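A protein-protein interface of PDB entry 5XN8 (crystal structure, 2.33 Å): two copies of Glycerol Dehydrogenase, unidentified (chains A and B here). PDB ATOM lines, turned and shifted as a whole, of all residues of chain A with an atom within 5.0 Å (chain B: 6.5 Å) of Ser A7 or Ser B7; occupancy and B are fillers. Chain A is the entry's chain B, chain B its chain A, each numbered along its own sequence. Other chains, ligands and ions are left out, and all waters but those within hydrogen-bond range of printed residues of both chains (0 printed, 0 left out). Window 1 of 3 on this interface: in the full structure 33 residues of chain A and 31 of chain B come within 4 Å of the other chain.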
ATOM      1  N   ILE A   5      15.255 -10.174 -18.439  1.00  0.00           N
ATOM      2  CA  ILE A   5      16.284 -10.409 -17.422  1.00  0.00           C
ATOM      3  C   ILE A   5      15.637 -11.235 -16.305  1.00  0.00           C
ATOM      4  O   ILE A   5      14.498 -10.973 -15.919  1.00  0.00           O
ATOM      5  CB  ILE A   5      16.888  -9.086 -16.879  1.00  0.00           C
ATOM      6  CG1 ILE A   5      17.986  -9.357 -15.844  1.00  0.00           C
ATOM      7  CG2 ILE A   5      15.824  -8.182 -16.270  1.00  0.00           C
ATOM      8  CD1 ILE A   5      18.798  -8.137 -15.470  1.00  0.00           C
ATOM      9  N   GLN A   6      16.347 -12.253 -15.820  1.00  0.00           N
ATOM     10  CA  GLN A   6      15.883 -13.005 -14.650  1.00  0.00           C
ATOM     11  C   GLN A   6      16.938 -13.019 -13.559  1.00  0.00           C
ATOM     12  O   GLN A   6      18.114 -12.728 -13.802  1.00  0.00           O
ATOM     13  CB  GLN A   6      15.385 -14.412 -15.012  1.00  0.00           C
ATOM     14  CG  GLN A   6      16.358 -15.351 -15.701  1.00  0.00           C
ATOM     15  CD  GLN A   6      15.687 -16.667 -16.080  1.00  0.00           C
ATOM     16  OE1 GLN A   6      14.845 -16.713 -16.976  1.00  0.00           O
ATOM     17  NE2 GLN A   6      16.046 -17.744 -15.383  1.00  0.00           N
ATOM     18  N   SER A   7      16.486 -13.301 -12.345  1.00  0.00           N
ATOM     19  CA  SER A   7      17.339 -13.223 -11.173  1.00  0.00           C
ATOM     20  C   SER A   7      16.827 -14.161 -10.081  1.00  0.00           C
ATOM     21  O   SER A   7      15.627 -14.471 -10.044  1.00  0.00           O
ATOM     22  CB  SER A   7      17.360 -11.776 -10.654  1.00  0.00           C
ATOM     23  OG  SER A   7      18.313 -11.593  -9.615  1.00  0.00           O
ATOM     24  N   PRO A   8      17.730 -14.630  -9.199  1.00  0.00           N
ATOM     25  CA  PRO A   8      17.240 -15.236  -7.961  1.00  0.00           C
ATOM     26  C   PRO A   8      16.575 -14.168  -7.092  1.00  0.00           C
ATOM     27  O   PRO A   8      17.033 -13.026  -7.088  1.00  0.00           O
ATOM     28  CB  PRO A   8      18.522 -15.743  -7.294  1.00  0.00           C
ATOM     29  CG  PRO A   8      19.590 -14.855  -7.825  1.00  0.00           C
ATOM     30  CD  PRO A   8      19.203 -14.650  -9.261  1.00  0.00           C
ATOM     31  N   GLY A   9      15.512 -14.537  -6.384  1.00  0.00           N
ATOM     32  CA  GLY A   9      14.769 -13.626  -5.508  1.00  0.00           C
ATOM     33  C   GLY A   9      15.628 -12.793  -4.568  1.00  0.00           C
ATOM     34  O   GLY A   9      15.442 -11.580  -4.471  1.00  0.00           O
ATOM     35  N   ASN A 146      14.567 -19.237 -10.987  1.00  0.00           N
ATOM     36  CA  ASN A 146      15.893 -19.232 -10.356  1.00  0.00           C
ATOM     37  C   ASN A 146      15.750 -19.653  -8.893  1.00  0.00           C
ATOM     38  O   ASN A 146      14.651 -19.630  -8.353  1.00  0.00           O
ATOM     39  CB  ASN A 146      16.530 -17.842 -10.412  1.00  0.00           C
ATOM     40  CG  ASN A 146      16.941 -17.444 -11.811  1.00  0.00           C
ATOM     41  OD1 ASN A 146      16.105 -17.215 -12.674  1.00  0.00           O
ATOM     42  ND2 ASN A 146      18.244 -17.340 -12.035  1.00  0.00           N
ATOM     43  N   TYR A 239      27.198 -13.384  -8.567  1.00  0.00           N
ATOM     44  CA  TYR A 239      26.036 -12.600  -8.982  1.00  0.00           C
ATOM     45  C   TYR A 239      26.250 -11.916 -10.339  1.00  0.00           C
ATOM     46  O   TYR A 239      25.392 -12.022 -11.222  1.00  0.00           O
ATOM     47  CB  TYR A 239      25.600 -11.585  -7.910  1.00  0.00           C
ATOM     48  CG  TYR A 239      24.200 -11.069  -8.169  1.00  0.00           C
ATOM     49  CD1 TYR A 239      23.072 -11.786  -7.748  1.00  0.00           C
ATOM     50  CD2 TYR A 239      23.988  -9.895  -8.885  1.00  0.00           C
ATOM     51  CE1 TYR A 239      21.791 -11.342  -8.028  1.00  0.00           C
ATOM     52  CE2 TYR A 239      22.713  -9.437  -9.165  1.00  0.00           C
ATOM     53  CZ  TYR A 239      21.619 -10.152  -8.739  1.00  0.00           C
ATOM     54  OH  TYR A 239      20.355  -9.671  -9.020  1.00  0.00           O
ATOM     55  N   ILE A 243      24.133 -13.411 -13.600  1.00  0.00           N
ATOM     56  CA  ILE A 243      23.152 -12.598 -14.340  1.00  0.00           C
ATOM     57  C   ILE A 243      23.679 -12.363 -15.755  1.00  0.00           C
ATOM     58  O   ILE A 243      22.921 -12.426 -16.727  1.00  0.00           O
ATOM     59  CB  ILE A 243      22.865 -11.226 -13.658  1.00  0.00           C
ATOM     60  CG1 ILE A 243      22.262 -11.396 -12.254  1.00  0.00           C
ATOM     61  CG2 ILE A 243      21.935 -10.366 -14.517  1.00  0.00           C
ATOM     62  CD1 ILE A 243      20.919 -12.091 -12.195  1.00  0.00           C
ATOM     63  N   ILE B   5      20.919  -8.118  -2.134  1.00  0.00           N
ATOM     64  CA  ILE B   5      20.220  -7.567  -3.298  1.00  0.00           C
ATOM     65  C   ILE B   5      18.998  -8.448  -3.554  1.00  0.00           C
ATOM     66  O   ILE B   5      19.085  -9.676  -3.459  1.00  0.00           O
ATOM     67  CB  ILE B   5      21.146  -7.494  -4.547  1.00  0.00           C
ATOM     68  CG1 ILE B   5      20.414  -6.884  -5.747  1.00  0.00           C
ATOM     69  CG2 ILE B   5      21.706  -8.866  -4.926  1.00  0.00           C
ATOM     70  CD1 ILE B   5      21.326  -6.538  -6.904  1.00  0.00           C
ATOM     71  N   GLN B   6      17.852  -7.827  -3.843  1.00  0.00           N
ATOM     72  CA  GLN B   6      16.664  -8.581  -4.251  1.00  0.00           C
ATOM     73  C   GLN B   6      16.136  -8.084  -5.583  1.00  0.00           C
ATOM     74  O   GLN B   6      16.480  -6.995  -6.040  1.00  0.00           O
ATOM     75  CB  GLN B   6      15.583  -8.619  -3.157  1.00  0.00           C
ATOM     76  CG  GLN B   6      15.028  -7.286  -2.669  1.00  0.00           C
ATOM     77  CD  GLN B   6      14.037  -7.480  -1.529  1.00  0.00           C
ATOM     78  OE1 GLN B   6      14.410  -7.880  -0.409  1.00  0.00           O
ATOM     79  NE2 GLN B   6      12.762  -7.235  -1.810  1.00  0.00           N
ATOM     80  N   SER B   7      15.341  -8.925  -6.228  1.00  0.00           N
ATOM     81  CA  SER B   7      14.865  -8.664  -7.575  1.00  0.00           C
ATOM     82  C   SER B   7      13.550  -9.393  -7.830  1.00  0.00           C
ATOM     83  O   SER B   7      13.281 -10.417  -7.192  1.00  0.00           O
ATOM     84  CB  SER B   7      15.922  -9.123  -8.591  1.00  0.00           C
ATOM     85  OG  SER B   7      15.600  -8.731  -9.923  1.00  0.00           O
ATOM     86  N   PRO B   8      12.713  -8.862  -8.744  1.00  0.00           N
ATOM     87  CA  PRO B   8      11.626  -9.695  -9.257  1.00  0.00           C
ATOM     88  C   PRO B   8      12.203 -10.843 -10.083  1.00  0.00           C
ATOM     89  O   PRO B   8      13.215 -10.651 -10.758  1.00  0.00           O
ATOM     90  CB  PRO B   8      10.850  -8.730 -10.164  1.00  0.00           C
ATOM     91  CG  PRO B   8      11.861  -7.723 -10.578  1.00  0.00           C
ATOM     92  CD  PRO B   8      12.688  -7.519  -9.348  1.00  0.00           C
ATOM     93  N   GLY B   9      11.572 -12.010 -10.017  1.00  0.00           N
ATOM     94  CA  GLY B   9      12.010 -13.207 -10.753  1.00  0.00           C
ATOM     95  C   GLY B   9      12.315 -12.973 -12.225  1.00  0.00           C
ATOM     96  O   GLY B   9      13.355 -13.410 -12.710  1.00  0.00           O
ATOM     97  N   LYS B  10      11.409 -12.281 -12.924  1.00  0.00           N
ATOM     98  CA  LYS B  10      11.573 -11.964 -14.348  1.00  0.00           C
ATOM     99  C   LYS B  10      11.037 -10.571 -14.659  1.00  0.00           C
ATOM    100  O   LYS B  10      10.003 -10.166 -14.132  1.00  0.00           O
ATOM    101  CB  LYS B  10      10.843 -12.986 -15.230  1.00  0.00           C
ATOM    102  CG  LYS B  10      11.508 -14.347 -15.301  1.00  0.00           C
ATOM    103  CD  LYS B  10      11.040 -15.160 -16.492  1.00  0.00           C
ATOM    104  CE  LYS B  10      11.403 -16.625 -16.322  1.00  0.00           C
ATOM    105  NZ  LYS B  10      10.581 -17.316 -15.284  1.00  0.00           N
ATOM    106  N   THR B 124       8.693  -2.942  -9.533  1.00  0.00           N
ATOM    107  CA  THR B 124       9.600  -4.051  -9.200  1.00  0.00           C
ATOM    108  C   THR B 124       9.734  -4.315  -7.695  1.00  0.00           C
ATOM    109  O   THR B 124      10.174  -5.404  -7.300  1.00  0.00           O
ATOM    110  CB  THR B 124      11.038  -3.812  -9.747  1.00  0.00           C
ATOM    111  OG1 THR B 124      11.627  -2.683  -9.092  1.00  0.00           O
ATOM    112  CG2 THR B 124      11.028  -3.562 -11.248  1.00  0.00           C
ATOM    113  N   LYS B 145       8.792 -11.028  -0.621  1.00  0.00           N
ATOM    114  CA  LYS B 145       8.984 -11.403  -2.018  1.00  0.00           C
ATOM    115  C   LYS B 145       8.660 -10.250  -2.975  1.00  0.00           C
ATOM    116  O   LYS B 145       7.698  -9.521  -2.759  1.00  0.00           O
ATOM    117  CB  LYS B 145       8.104 -12.615  -2.340  1.00  0.00           C
ATOM    118  CG  LYS B 145       8.590 -13.414  -3.541  1.00  0.00           C
ATOM    119  CD  LYS B 145       7.659 -14.556  -3.887  1.00  0.00           C
ATOM    120  CE  LYS B 145       7.748 -15.655  -2.843  1.00  0.00           C
ATOM    121  NZ  LYS B 145       7.283 -16.981  -3.365  1.00  0.00           N
ATOM    122  N   ASN B 146       9.472 -10.094  -4.022  1.00  0.00           N
ATOM    123  CA  ASN B 146       9.166  -9.167  -5.119  1.00  0.00           C
ATOM    124  C   ASN B 146       8.137  -9.810  -6.048  1.00  0.00           C
ATOM    125  O   ASN B 146       7.928 -11.022  -5.990  1.00  0.00           O
ATOM    126  CB  ASN B 146      10.419  -8.831  -5.928  1.00  0.00           C
ATOM    127  CG  ASN B 146      11.395  -7.968  -5.166  1.00  0.00           C
ATOM    128  OD1 ASN B 146      12.009  -8.410  -4.194  1.00  0.00           O
ATOM    129  ND2 ASN B 146      11.559  -6.728  -5.617  1.00  0.00           N
ATOM    130  N   PRO B 147       7.477  -9.008  -6.907  1.00  0.00           N
ATOM    131  CA  PRO B 147       6.623  -9.610  -7.936  1.00  0.00           C
ATOM    132  C   PRO B 147       7.362 -10.681  -8.734  1.00  0.00           C
ATOM    133  O   PRO B 147       8.548 -10.530  -9.023  1.00  0.00           O
ATOM    134  CB  PRO B 147       6.286  -8.431  -8.841  1.00  0.00           C
ATOM    135  CG  PRO B 147       6.327  -7.258  -7.935  1.00  0.00           C
ATOM    136  CD  PRO B 147       7.402  -7.536  -6.932  1.00  0.00           C
ATOM    137  N   TYR B 239      13.367  -0.867 -13.974  1.00  0.00           N
ATOM    138  CA  TYR B 239      14.270  -1.887 -13.431  1.00  0.00           C
ATOM    139  C   TYR B 239      15.487  -1.271 -12.739  1.00  0.00           C
ATOM    140  O   TYR B 239      15.805  -1.656 -11.615  1.00  0.00           O
ATOM    141  CB  TYR B 239      14.699  -2.910 -14.508  1.00  0.00           C
ATOM    142  CG  TYR B 239      15.328  -4.143 -13.893  1.00  0.00           C
ATOM    143  CD1 TYR B 239      16.678  -4.167 -13.567  1.00  0.00           C
ATOM    144  CD2 TYR B 239      14.563  -5.262 -13.584  1.00  0.00           C
ATOM    145  CE1 TYR B 239      17.258  -5.295 -12.975  1.00  0.00           C
ATOM    146  CE2 TYR B 239      15.126  -6.382 -12.987  1.00  0.00           C
ATOM    147  CZ  TYR B 239      16.468  -6.400 -12.685  1.00  0.00           C
ATOM    148  OH  TYR B 239      17.007  -7.517 -12.095  1.00  0.00           O
ATOM    149  N   ILE B 243      15.646  -1.559  -8.596  1.00  0.00           N
ATOM    150  CA  ILE B 243      16.722  -2.297  -7.898  1.00  0.00           C
ATOM    151  C   ILE B 243      17.561  -1.290  -7.114  1.00  0.00           C
ATOM    152  O   ILE B 243      17.955  -1.553  -5.983  1.00  0.00           O
ATOM    153  CB  ILE B 243      17.638  -3.089  -8.874  1.00  0.00           C
ATOM    154  CG1 ILE B 243      16.873  -4.164  -9.661  1.00  0.00           C
ATOM    155  CG2 ILE B 243      18.812  -3.727  -8.134  1.00  0.00           C
ATOM    156  CD1 ILE B 243      16.237  -5.254  -8.836  1.00  0.00           C
ATOM    157  N   GLU B 246      15.589  -0.017  -3.687  1.00  0.00           N
ATOM    158  CA  GLU B 246      15.244  -1.080  -2.744  1.00  0.00           C
ATOM    159  C   GLU B 246      16.465  -1.792  -2.173  1.00  0.00           C
ATOM    160  O   GLU B 246      16.475  -2.137  -0.987  1.00  0.00           O
ATOM    161  CB  GLU B 246      14.312  -2.099  -3.407  1.00  0.00           C
ATOM    162  CG  GLU B 246      13.740  -3.133  -2.445  1.00  0.00           C
ATOM    163  CD  GLU B 246      12.728  -4.040  -3.108  1.00  0.00           C
ATOM    164  OE1 GLU B 246      13.081  -4.704  -4.114  1.00  0.00           O
ATOM    165  OE2 GLU B 246      11.574  -4.089  -2.619  1.00  0.00           O
ATOM    166  N   SER B 247      17.472  -2.032  -3.021  1.00  0.00           N
ATOM    167  CA  SER B 247      18.672  -2.785  -2.646  1.00  0.00           C
ATOM    168  C   SER B 247      19.946  -1.944  -2.468  1.00  0.00           C
ATOM    169  O   SER B 247      20.966  -2.470  -2.006  1.00  0.00           O
ATOM    170  CB  SER B 247      18.926  -3.893  -3.673  1.00  0.00           C
ATOM    171  OG  SER B 247      17.865  -4.836  -3.665  1.00  0.00           O
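The backbone NH (N) of Ser A7 lies within hydrogen-bond range of the backbone carbonyl oxygen (O) of Gly B9, at 3.2 Å.
N of Ser B7 is in hydrogen-bond range of O of Gly A9, at 3.2 Å.
OG of Ser A7 is in hydrogen-bond range of OH of Tyr A239, 2.9 Å away.
NE2 of Gln B6 lies within hydrogen-bond range of OD1 of Asn B146.
The side-chain hydroxyl (OH) of Tyr B239 lies within hydrogen-bond range of the side-chain hydroxyl (OG) of Ser B7, 2.9 Å away.
NE2 of Gln B6 is in hydrogen-bond range of OE1 of Glu B246.
OD1 of Asn A146 sits at hydrogen-bond distance from NE2 of Gln A6, 2.8 Å away.
The backbone NH (N) of Gln B6 is in hydrogen-bond range of the side-chain hydroxyl (OG) of Ser B247.
Ile A5 touches Lys B10.
CE2 of Tyr B239 touches CG2 of Ile A5, 3.8 Å away.
Gln A6 touches Gly B9 (CA to O, 3.2 Å).
Lys B10 touches Gln A6.
Ser B7 touches Ser A7 (CB to OG, 3.6 Å).
O of Gly A9 touches CB of Gln B6, 3.2 Å away.
CD1 of Ile B5 touches OH of Tyr A239 (3.9 Å).
Ser A7 touches just these residues of chain B: Ser B7 and Gly B9.
Ser B7 touches just these residues of chain A: Ser A7 and Gly A9.
Printed residues of chain A within 4 Å of Lys B10: Ile A5 and Gln A6.
Of the printed residues of chain A, Gln B6 touches Gly A9 (3.2 Å).
Printed residues of chain A within 4 Å of Tyr B239: Ile A5 (3.8 Å).
Ser B247 touches none of the printed residues of chain A.
Pro B8 touches none of the printed residues of chain A.
The nearest residue of chain B that does not touch Ser A7 is Pro B8 (4.3 Å).
Of the 8 printed residues of chain A, 5 touch a printed residue of chain B.
Hydrophobic or aromatic side chains of chain A within 4 Å of the printed part of chain B: Ile A5 and Tyr A239.
Of the 14 printed residues of chain B, 6 touch a printed residue of chain A.
Hydrophobic or aromatic side chains of chain B within 4 Å of the printed part of chain A: Ile B5 and Tyr B239.
Among the printed residues, no Asp or Glu carboxylate lies within 4 Å of a Lys or Arg side-chain nitrogen of the other chain.
Ile A5 touches Tyr B239, and with the chains exchanged Tyr A239 touches Ile B5.
Gln A6 touches Gly B9, and with the chains exchanged Gly A9 touches Gln B6.
Ser B7 touches its own counterpart, Ser A7.
Ser A7 touches Gly B9, and with the chains exchanged Gly A9 touches Ser B7.
8 positions are printed for both chains.
Of the 9 pairs that touch across the chains among the printed residues, 7 have their exchanged pair printed and touching as well.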
